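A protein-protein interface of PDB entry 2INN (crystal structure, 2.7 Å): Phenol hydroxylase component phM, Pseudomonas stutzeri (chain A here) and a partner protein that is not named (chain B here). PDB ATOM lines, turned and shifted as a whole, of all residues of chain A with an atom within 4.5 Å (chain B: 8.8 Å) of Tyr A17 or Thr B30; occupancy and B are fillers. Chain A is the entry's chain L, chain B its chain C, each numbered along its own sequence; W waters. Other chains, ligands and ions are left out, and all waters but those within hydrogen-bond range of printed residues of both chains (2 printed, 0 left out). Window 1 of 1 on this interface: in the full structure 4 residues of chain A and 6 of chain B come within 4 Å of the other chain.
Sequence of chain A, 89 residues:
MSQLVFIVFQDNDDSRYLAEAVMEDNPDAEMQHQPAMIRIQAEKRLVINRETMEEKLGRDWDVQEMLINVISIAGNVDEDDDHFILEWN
The side-chain carboxylate (OD1) of Asp A13 lies within salt-bridge range of the guanidinium group (NE) of Arg B31, at 3.7 Å.
The backbone NH of Thr B30 lies within hydrogen-bond range of the side-chain amide oxygen of Gln B33 (2.8 Å).
Among the printed residues, merely in contact across the chains: Arg A16 with Pro B28 (3.5 Å), Tyr A17 with Thr B30 (3.5 Å) and Arg A16 with Ala B29 (3.6 Å).
Tyr A17 touches just one residue of chain B: Thr B30.
Thr B30 touches just one residue of chain A: Tyr A17 (3.5 Å).
Printed residues of chain A within 4 Å of Pro B28: Arg A16.
Of the printed residues of chain B, Arg A16 touches Pro B28 and Ala B29.
Printed residues of chain A within 4 Å of Arg B31: Asp A13.
Of the printed residues of chain A, Ala B29 touches Arg A16.
Printed residues of chain B within 4 Å of Asp A13: Arg B31 (3.7 Å).
Of the 10 printed residues of chain A, 3 touch a printed residue of chain B.
Hydrophobic or aromatic side chains of chain B that line the printed part of chain A: Pro B28.
Along chain B the printed residues that touch a printed residue of chain A span positions 28 to 31.
Among the printed residues, 4 pairs touch across the chains.
Among the printed residues, Asp or Glu carboxylates within 4 Å of a Lys or Arg side-chain nitrogen of the other chain: Asp A13 with Arg B31 (3.7 Å).
Water W1 lies within hydrogen-bond range of OD1 of Asp A13 (2.5 Å) and O of Ala B29 (3.3 Å).
Water W2 lies within hydrogen-bond range of OH of Tyr A17 (2.6 Å), OD2 of Asp A13 (2.7 Å) and N of Arg B31 (3.0 Å).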
ATOM      1  N   ASP A  13      13.566 -20.449  24.801  1.00  0.00           N
ATOM      2  CA  ASP A  13      14.071 -19.098  24.527  1.00  0.00           C
ATOM      3  C   ASP A  13      15.093 -19.168  23.374  1.00  0.00           C
ATOM      4  O   ASP A  13      15.015 -18.411  22.375  1.00  0.00           O
ATOM      5  CB  ASP A  13      14.699 -18.509  25.784  1.00  0.00           C
ATOM      6  CG  ASP A  13      15.154 -17.086  25.587  1.00  0.00           C
ATOM      7  OD1 ASP A  13      14.361 -16.133  25.813  1.00  0.00           O
ATOM      8  OD2 ASP A  13      16.337 -16.936  25.221  1.00  0.00           O
ATOM      9  N   ASP A  14      16.036 -20.102  23.522  1.00  0.00           N
ATOM     10  CA  ASP A  14      17.125 -20.337  22.558  1.00  0.00           C
ATOM     11  C   ASP A  14      16.626 -20.826  21.238  1.00  0.00           C
ATOM     12  O   ASP A  14      17.244 -20.576  20.198  1.00  0.00           O
ATOM     13  CB  ASP A  14      18.105 -21.390  23.077  1.00  0.00           C
ATOM     14  CG  ASP A  14      18.394 -21.206  24.516  1.00  0.00           C
ATOM     15  OD1 ASP A  14      19.510 -20.710  24.808  1.00  0.00           O
ATOM     16  OD2 ASP A  14      17.471 -21.489  25.336  1.00  0.00           O
ATOM     17  N   SER A  15      15.532 -21.570  21.313  1.00  0.00           N
ATOM     18  CA  SER A  15      14.948 -22.227  20.164  1.00  0.00           C
ATOM     19  C   SER A  15      14.204 -21.226  19.243  1.00  0.00           C
ATOM     20  O   SER A  15      14.059 -21.438  18.029  1.00  0.00           O
ATOM     21  CB  SER A  15      14.076 -23.372  20.641  1.00  0.00           C
ATOM     22  OG  SER A  15      14.911 -24.444  21.058  1.00  0.00           O
ATOM     23  N   ARG A  16      13.794 -20.103  19.805  1.00  0.00           N
ATOM     24  CA  ARG A  16      13.294 -19.072  18.945  1.00  0.00           C
ATOM     25  C   ARG A  16      14.332 -18.823  17.845  1.00  0.00           C
ATOM     26  O   ARG A  16      13.979 -18.685  16.659  1.00  0.00           O
ATOM     27  CB  ARG A  16      13.024 -17.797  19.732  1.00  0.00           C
ATOM     28  CG  ARG A  16      12.004 -16.900  19.058  1.00  0.00           C
ATOM     29  CD  ARG A  16      12.053 -15.551  19.679  1.00  0.00           C
ATOM     30  NE  ARG A  16      11.355 -15.597  20.947  1.00  0.00           N
ATOM     31  CZ  ARG A  16      11.766 -14.928  22.019  1.00  0.00           C
ATOM     32  NH1 ARG A  16      12.886 -14.182  21.974  1.00  0.00           N
ATOM     33  NH2 ARG A  16      11.058 -14.996  23.131  1.00  0.00           N
ATOM     34  N   TYR A  17      15.604 -18.793  18.245  1.00  0.00           N
ATOM     35  CA  TYR A  17      16.691 -18.348  17.376  1.00  0.00           C
ATOM     36  C   TYR A  17      17.039 -19.473  16.502  1.00  0.00           C
ATOM     37  O   TYR A  17      17.481 -19.267  15.377  1.00  0.00           O
ATOM     38  CB  TYR A  17      17.921 -17.935  18.168  1.00  0.00           C
ATOM     39  CG  TYR A  17      17.559 -16.904  19.185  1.00  0.00           C
ATOM     40  CD1 TYR A  17      17.268 -15.589  18.786  1.00  0.00           C
ATOM     41  CD2 TYR A  17      17.440 -17.247  20.542  1.00  0.00           C
ATOM     42  CE1 TYR A  17      16.886 -14.628  19.703  1.00  0.00           C
ATOM     43  CE2 TYR A  17      17.075 -16.302  21.481  1.00  0.00           C
ATOM     44  CZ  TYR A  17      16.805 -14.977  21.069  1.00  0.00           C
ATOM     45  OH  TYR A  17      16.449 -14.006  22.004  1.00  0.00           O
ATOM     46  N   LEU A  18      16.835 -20.682  17.017  1.00  0.00           N
ATOM     47  CA  LEU A  18      17.185 -21.869  16.245  1.00  0.00           C
ATOM     48  C   LEU A  18      16.100 -22.067  15.187  1.00  0.00           C
ATOM     49  O   LEU A  18      16.434 -22.403  14.057  1.00  0.00           O
ATOM     50  CB  LEU A  18      17.404 -23.122  17.130  1.00  0.00           C
ATOM     51  CG  LEU A  18      18.366 -23.182  18.355  1.00  0.00           C
ATOM     52  CD1 LEU A  18      18.111 -24.399  19.256  1.00  0.00           C
ATOM     53  CD2 LEU A  18      19.847 -23.160  17.993  1.00  0.00           C
ATOM     54  N   ALA A  19      14.829 -21.820  15.554  1.00  0.00           N
ATOM     55  CA  ALA A  19      13.674 -21.786  14.625  1.00  0.00           C
ATOM     56  C   ALA A  19      13.878 -20.772  13.515  1.00  0.00           C
ATOM     57  O   ALA A  19      14.060 -21.133  12.347  1.00  0.00           O
ATOM     58  CB  ALA A  19      12.418 -21.405  15.369  1.00  0.00           C
ATOM     59  N   GLU A  20      13.765 -19.498  13.881  1.00  0.00           N
ATOM     60  CA  GLU A  20      14.313 -18.412  13.080  1.00  0.00           C
ATOM     61  C   GLU A  20      15.290 -18.906  11.983  1.00  0.00           C
ATOM     62  O   GLU A  20      14.853 -19.190  10.868  1.00  0.00           O
ATOM     63  CB  GLU A  20      14.995 -17.406  14.013  1.00  0.00           C
ATOM     64  CG  GLU A  20      14.781 -15.943  13.677  1.00  0.00           C
ATOM     65  CD  GLU A  20      14.229 -15.192  14.855  1.00  0.00           C
ATOM     66  OE1 GLU A  20      13.079 -15.472  15.226  1.00  0.00           O
ATOM     67  OE2 GLU A  20      14.941 -14.320  15.402  1.00  0.00           O
ATOM     68  N   ALA A  21      16.586 -19.034  12.297  1.00  0.00           N
ATOM     69  CA  ALA A  21      17.638 -19.475  11.342  1.00  0.00           C
ATOM     70  C   ALA A  21      17.251 -20.575  10.330  1.00  0.00           C
ATOM     71  O   ALA A  21      17.725 -20.573   9.190  1.00  0.00           O
ATOM     72  CB  ALA A  21      18.905 -19.893  12.089  1.00  0.00           C
ATOM     73  N   MET A  53      23.033 -18.402  11.851  1.00  0.00           N
ATOM     74  CA  MET A  53      23.074 -18.368  13.299  1.00  0.00           C
ATOM     75  C   MET A  53      24.068 -17.386  13.939  1.00  0.00           C
ATOM     76  O   MET A  53      23.696 -16.633  14.844  1.00  0.00           O
ATOM     77  CB  MET A  53      23.349 -19.796  13.814  1.00  0.00           C
ATOM     78  CG  MET A  53      22.632 -20.165  15.135  1.00  0.00           C
ATOM     79  SD  MET A  53      20.742 -20.700  14.906  1.00  0.00           S
ATOM     80  CE  MET A  53      21.019 -22.473  13.874  1.00  0.00           C
ATOM     81  N   HIS B  15       3.888  -8.887  23.337  1.00  0.00           N
ATOM     82  CA  HIS B  15       5.109  -9.653  23.305  1.00  0.00           C
ATOM     83  C   HIS B  15       6.232  -9.273  24.206  1.00  0.00           C
ATOM     84  O   HIS B  15       7.113 -10.063  24.364  1.00  0.00           O
ATOM     85  CB  HIS B  15       5.618  -9.659  21.939  1.00  0.00           C
ATOM     86  CG  HIS B  15       4.633 -10.241  21.020  1.00  0.00           C
ATOM     87  ND1 HIS B  15       4.527 -11.601  20.836  1.00  0.00           N
ATOM     88  CD2 HIS B  15       3.657  -9.666  20.274  1.00  0.00           C
ATOM     89  CE1 HIS B  15       3.534 -11.831  19.989  1.00  0.00           C
ATOM     90  NE2 HIS B  15       2.993 -10.678  19.635  1.00  0.00           N
ATOM     91  N   THR B  16       6.200  -8.094  24.774  1.00  0.00           N
ATOM     92  CA  THR B  16       7.309  -7.650  25.538  1.00  0.00           C
ATOM     93  C   THR B  16       6.869  -6.423  26.291  1.00  0.00           C
ATOM     94  O   THR B  16       5.681  -6.080  26.266  1.00  0.00           O
ATOM     95  CB  THR B  16       8.449  -7.283  24.625  1.00  0.00           C
ATOM     96  OG1 THR B  16       9.575  -7.017  25.414  1.00  0.00           O
ATOM     97  CG2 THR B  16       8.127  -6.066  23.881  1.00  0.00           C
ATOM     98  N   TYR B  17       7.785  -5.772  26.985  1.00  0.00           N
ATOM     99  CA  TYR B  17       7.364  -4.607  27.742  1.00  0.00           C
ATOM    100  C   TYR B  17       7.365  -3.334  26.882  1.00  0.00           C
ATOM    101  O   TYR B  17       8.123  -3.132  25.919  1.00  0.00           O
ATOM    102  CB  TYR B  17       8.254  -4.333  28.938  1.00  0.00           C
ATOM    103  CG  TYR B  17       8.426  -5.420  29.935  1.00  0.00           C
ATOM    104  CD1 TYR B  17       9.433  -6.362  29.779  1.00  0.00           C
ATOM    105  CD2 TYR B  17       7.676  -5.420  31.104  1.00  0.00           C
ATOM    106  CE1 TYR B  17       9.647  -7.309  30.728  1.00  0.00           C
ATOM    107  CE2 TYR B  17       7.870  -6.360  32.081  1.00  0.00           C
ATOM    108  CZ  TYR B  17       8.842  -7.322  31.904  1.00  0.00           C
ATOM    109  OH  TYR B  17       9.035  -8.315  32.882  1.00  0.00           O
ATOM    110  N   ILE B  20      10.417  -1.556  25.599  1.00  0.00           N
ATOM    111  CA  ILE B  20      11.040  -2.352  24.566  1.00  0.00           C
ATOM    112  C   ILE B  20      10.281  -2.317  23.283  1.00  0.00           C
ATOM    113  O   ILE B  20      10.872  -2.164  22.245  1.00  0.00           O
ATOM    114  CB  ILE B  20      11.209  -3.898  24.999  1.00  0.00           C
ATOM    115  CG1 ILE B  20      11.679  -3.974  26.437  1.00  0.00           C
ATOM    116  CG2 ILE B  20      12.249  -4.612  24.104  1.00  0.00           C
ATOM    117  CD1 ILE B  20      12.998  -3.140  26.578  1.00  0.00           C
ATOM    118  N   PHE B  24      12.046  -1.477  19.656  1.00  0.00           N
ATOM    119  CA  PHE B  24      12.431  -2.520  18.744  1.00  0.00           C
ATOM    120  C   PHE B  24      11.229  -3.214  18.132  1.00  0.00           C
ATOM    121  O   PHE B  24      11.401  -4.343  17.574  1.00  0.00           O
ATOM    122  CB  PHE B  24      13.230  -3.658  19.423  1.00  0.00           C
ATOM    123  CG  PHE B  24      14.423  -3.229  20.244  1.00  0.00           C
ATOM    124  CD1 PHE B  24      14.307  -3.078  21.609  1.00  0.00           C
ATOM    125  CD2 PHE B  24      15.664  -3.074  19.647  1.00  0.00           C
ATOM    126  CE1 PHE B  24      15.417  -2.686  22.375  1.00  0.00           C
ATOM    127  CE2 PHE B  24      16.763  -2.696  20.348  1.00  0.00           C
ATOM    128  CZ  PHE B  24      16.657  -2.495  21.750  1.00  0.00           C
ATOM    129  N   LYS B  27       7.266  -7.364  19.364  1.00  0.00           N
ATOM    130  CA  LYS B  27       7.498  -8.805  19.183  1.00  0.00           C
ATOM    131  C   LYS B  27       8.482  -9.189  20.208  1.00  0.00           C
ATOM    132  O   LYS B  27       9.243  -8.317  20.731  1.00  0.00           O
ATOM    133  CB  LYS B  27       8.076  -9.194  17.822  1.00  0.00           C
ATOM    134  CG  LYS B  27       8.989  -8.148  17.152  1.00  0.00           C
ATOM    135  CD  LYS B  27      10.442  -8.284  17.566  1.00  0.00           C
ATOM    136  CE  LYS B  27      11.283  -7.551  16.561  1.00  0.00           C
ATOM    137  NZ  LYS B  27      12.187  -8.599  16.051  1.00  0.00           N
ATOM    138  N   PRO B  28       8.508 -10.487  20.486  1.00  0.00           N
ATOM    139  CA  PRO B  28       9.289 -11.074  21.528  1.00  0.00           C
ATOM    140  C   PRO B  28      10.689 -10.385  21.604  1.00  0.00           C
ATOM    141  O   PRO B  28      11.368 -10.263  20.594  1.00  0.00           O
ATOM    142  CB  PRO B  28       9.419 -12.544  21.058  1.00  0.00           C
ATOM    143  CG  PRO B  28       8.539 -12.723  19.868  1.00  0.00           C
ATOM    144  CD  PRO B  28       7.780 -11.489  19.691  1.00  0.00           C
ATOM    145  N   ALA B  29      11.126  -9.931  22.781  1.00  0.00           N
ATOM    146  CA  ALA B  29      12.442  -9.253  22.782  1.00  0.00           C
ATOM    147  C   ALA B  29      13.571 -10.181  23.337  1.00  0.00           C
ATOM    148  O   ALA B  29      13.239 -11.202  23.927  1.00  0.00           O
ATOM    149  CB  ALA B  29      12.377  -7.874  23.461  1.00  0.00           C
ATOM    150  N   THR B  30      14.852  -9.912  23.084  1.00  0.00           N
ATOM    151  CA  THR B  30      15.853 -10.864  23.544  1.00  0.00           C
ATOM    152  C   THR B  30      16.008 -10.747  25.054  1.00  0.00           C
ATOM    153  O   THR B  30      15.716  -9.674  25.633  1.00  0.00           O
ATOM    154  CB  THR B  30      17.207 -10.596  22.896  1.00  0.00           C
ATOM    155  OG1 THR B  30      17.781  -9.384  23.444  1.00  0.00           O
ATOM    156  CG2 THR B  30      17.051 -10.457  21.405  1.00  0.00           C
ATOM    157  N   ARG B  31      16.489 -11.796  25.730  1.00  0.00           N
ATOM    158  CA  ARG B  31      16.889 -11.630  27.212  1.00  0.00           C
ATOM    159  C   ARG B  31      17.767 -10.444  27.502  1.00  0.00           C
ATOM    160  O   ARG B  31      17.474  -9.707  28.475  1.00  0.00           O
ATOM    161  CB  ARG B  31      17.570 -12.868  27.811  1.00  0.00           C
ATOM    162  CG  ARG B  31      16.668 -14.147  27.845  1.00  0.00           C
ATOM    163  CD  ARG B  31      16.315 -14.601  29.260  1.00  0.00           C
ATOM    164  NE  ARG B  31      15.558 -15.858  29.336  1.00  0.00           N
ATOM    165  CZ  ARG B  31      14.261 -15.869  29.687  1.00  0.00           C
ATOM    166  NH1 ARG B  31      13.614 -14.719  29.998  1.00  0.00           N
ATOM    167  NH2 ARG B  31      13.593 -17.036  29.777  1.00  0.00           N
ATOM    168  N   TYR B  32      18.812 -10.244  26.677  1.00  0.00           N
ATOM    169  CA  TYR B  32      19.645  -9.039  26.826  1.00  0.00           C
ATOM    170  C   TYR B  32      18.791  -7.766  26.730  1.00  0.00           C
ATOM    171  O   TYR B  32      19.002  -6.756  27.483  1.00  0.00           O
ATOM    172  CB  TYR B  32      20.842  -9.004  25.849  1.00  0.00           C
ATOM    173  CG  TYR B  32      21.674  -7.681  25.823  1.00  0.00           C
ATOM    174  CD1 TYR B  32      22.767  -7.477  26.702  1.00  0.00           C
ATOM    175  CD2 TYR B  32      21.417  -6.656  24.907  1.00  0.00           C
ATOM    176  CE1 TYR B  32      23.569  -6.281  26.647  1.00  0.00           C
ATOM    177  CE2 TYR B  32      22.199  -5.435  24.851  1.00  0.00           C
ATOM    178  CZ  TYR B  32      23.264  -5.227  25.723  1.00  0.00           C
ATOM    179  OH  TYR B  32      24.036  -3.998  25.715  1.00  0.00           O
ATOM    180  N   GLN B  33      17.814  -7.760  25.796  1.00  0.00           N
ATOM    181  CA  GLN B  33      17.036  -6.501  25.611  1.00  0.00           C
ATOM    182  C   GLN B  33      16.141  -6.222  26.813  1.00  0.00           C
ATOM    183  O   GLN B  33      16.195  -5.186  27.399  1.00  0.00           O
ATOM    184  CB  GLN B  33      16.277  -6.442  24.291  1.00  0.00           C
ATOM    185  CG  GLN B  33      17.195  -6.258  23.158  1.00  0.00           C
ATOM    186  CD  GLN B  33      16.510  -6.644  21.852  1.00  0.00           C
ATOM    187  OE1 GLN B  33      15.585  -7.478  21.855  1.00  0.00           O
ATOM    188  NE2 GLN B  33      17.000  -6.074  20.722  1.00  0.00           N
ATOM    189  N   GLU B  34      15.374  -7.175  27.252  1.00  0.00           N
ATOM    190  CA  GLU B  34      14.566  -6.880  28.409  1.00  0.00           C
ATOM    191  C   GLU B  34      15.353  -6.554  29.686  1.00  0.00           C
ATOM    192  O   GLU B  34      14.760  -6.012  30.585  1.00  0.00           O
ATOM    193  CB  GLU B  34      13.604  -8.058  28.580  1.00  0.00           C
ATOM    194  CG  GLU B  34      12.479  -8.045  27.559  1.00  0.00           C
ATOM    195  CD  GLU B  34      11.467  -9.158  27.806  1.00  0.00           C
ATOM    196  OE1 GLU B  34      11.647 -10.087  28.669  1.00  0.00           O
ATOM    197  OE2 GLU B  34      10.442  -9.123  27.066  1.00  0.00           O
ATOM    198  N   ALA B  35      16.649  -6.925  29.779  1.00  0.00           N
ATOM    199  CA  ALA B  35      17.434  -6.635  30.969  1.00  0.00           C
ATOM    200  C   ALA B  35      18.137  -5.262  30.865  1.00  0.00           C
ATOM    201  O   ALA B  35      18.427  -4.646  31.886  1.00  0.00           O
ATOM    202  CB  ALA B  35      18.482  -7.683  31.227  1.00  0.00           C
ATOM    203  N   SER B  36      18.425  -4.778  29.662  1.00  0.00           N
ATOM    204  CA  SER B  36      19.339  -3.640  29.536  1.00  0.00           C
ATOM    205  C   SER B  36      18.831  -2.194  29.187  1.00  0.00           C
ATOM    206  O   SER B  36      19.487  -1.205  29.533  1.00  0.00           O
ATOM    207  CB  SER B  36      20.477  -4.035  28.605  1.00  0.00           C
ATOM    208  OG  SER B  36      20.981  -5.324  28.936  1.00  0.00           O
ATOM    209  N   TYR B  37      17.661  -2.064  28.541  1.00  0.00           N
ATOM    210  CA  TYR B  37      17.187  -0.757  27.973  1.00  0.00           C
ATOM    211  C   TYR B  37      16.091  -0.228  28.814  1.00  0.00           C
ATOM    212  O   TYR B  37      15.186  -0.936  29.113  1.00  0.00           O
ATOM    213  CB  TYR B  37      16.657  -0.988  26.599  1.00  0.00           C
ATOM    214  CG  TYR B  37      17.722  -1.432  25.618  1.00  0.00           C
ATOM    215  CD1 TYR B  37      18.145  -2.770  25.519  1.00  0.00           C
ATOM    216  CD2 TYR B  37      18.313  -0.536  24.773  1.00  0.00           C
ATOM    217  CE1 TYR B  37      19.126  -3.169  24.576  1.00  0.00           C
ATOM    218  CE2 TYR B  37      19.260  -0.926  23.844  1.00  0.00           C
ATOM    219  CZ  TYR B  37      19.660  -2.220  23.751  1.00  0.00           C
ATOM    220  OH  TYR B  37      20.598  -2.509  22.795  1.00  0.00           O
ATOM    221  N   GLN B  78      26.561  -8.857  24.522  1.00  0.00           N
ATOM    222  CA  GLN B  78      25.201  -9.120  24.927  1.00  0.00           C
ATOM    223  C   GLN B  78      25.196  -9.566  26.446  1.00  0.00           C
ATOM    224  O   GLN B  78      24.299 -10.278  26.898  1.00  0.00           O
ATOM    225  CB  GLN B  78      24.599 -10.236  24.012  1.00  0.00           C
ATOM    226  CG  GLN B  78      24.331  -9.880  22.522  1.00  0.00           C
ATOM    227  CD  GLN B  78      23.028  -9.052  22.415  1.00  0.00           C
ATOM    228  OE1 GLN B  78      23.072  -7.797  22.525  1.00  0.00           O
ATOM    229  NE2 GLN B  78      21.836  -9.752  22.302  1.00  0.00           N
ATOM    230  N   TYR B  80      23.926  -9.411  29.787  1.00  0.00           N
ATOM    231  CA  TYR B  80      23.217  -9.093  31.012  1.00  0.00           C
ATOM    232  C   TYR B  80      23.828 -10.024  32.122  1.00  0.00           C
ATOM    233  O   TYR B  80      24.686 -10.966  31.843  1.00  0.00           O
ATOM    234  CB  TYR B  80      21.726  -9.293  30.879  1.00  0.00           C
ATOM    235  CG  TYR B  80      21.388 -10.739  30.565  1.00  0.00           C
ATOM    236  CD1 TYR B  80      20.875 -11.637  31.562  1.00  0.00           C
ATOM    237  CD2 TYR B  80      21.647 -11.232  29.277  1.00  0.00           C
ATOM    238  CE1 TYR B  80      20.586 -12.957  31.256  1.00  0.00           C
ATOM    239  CE2 TYR B  80      21.387 -12.517  28.934  1.00  0.00           C
ATOM    240  CZ  TYR B  80      20.859 -13.424  29.907  1.00  0.00           C
ATOM    241  OH  TYR B  80      20.633 -14.784  29.437  1.00  0.00           O
HETATM  242  O   HOH W   1      13.580 -13.743  26.033  1.00  0.00           O
HETATM  243  O   HOH W   2      17.036 -14.425  24.478  1.00  0.00           O
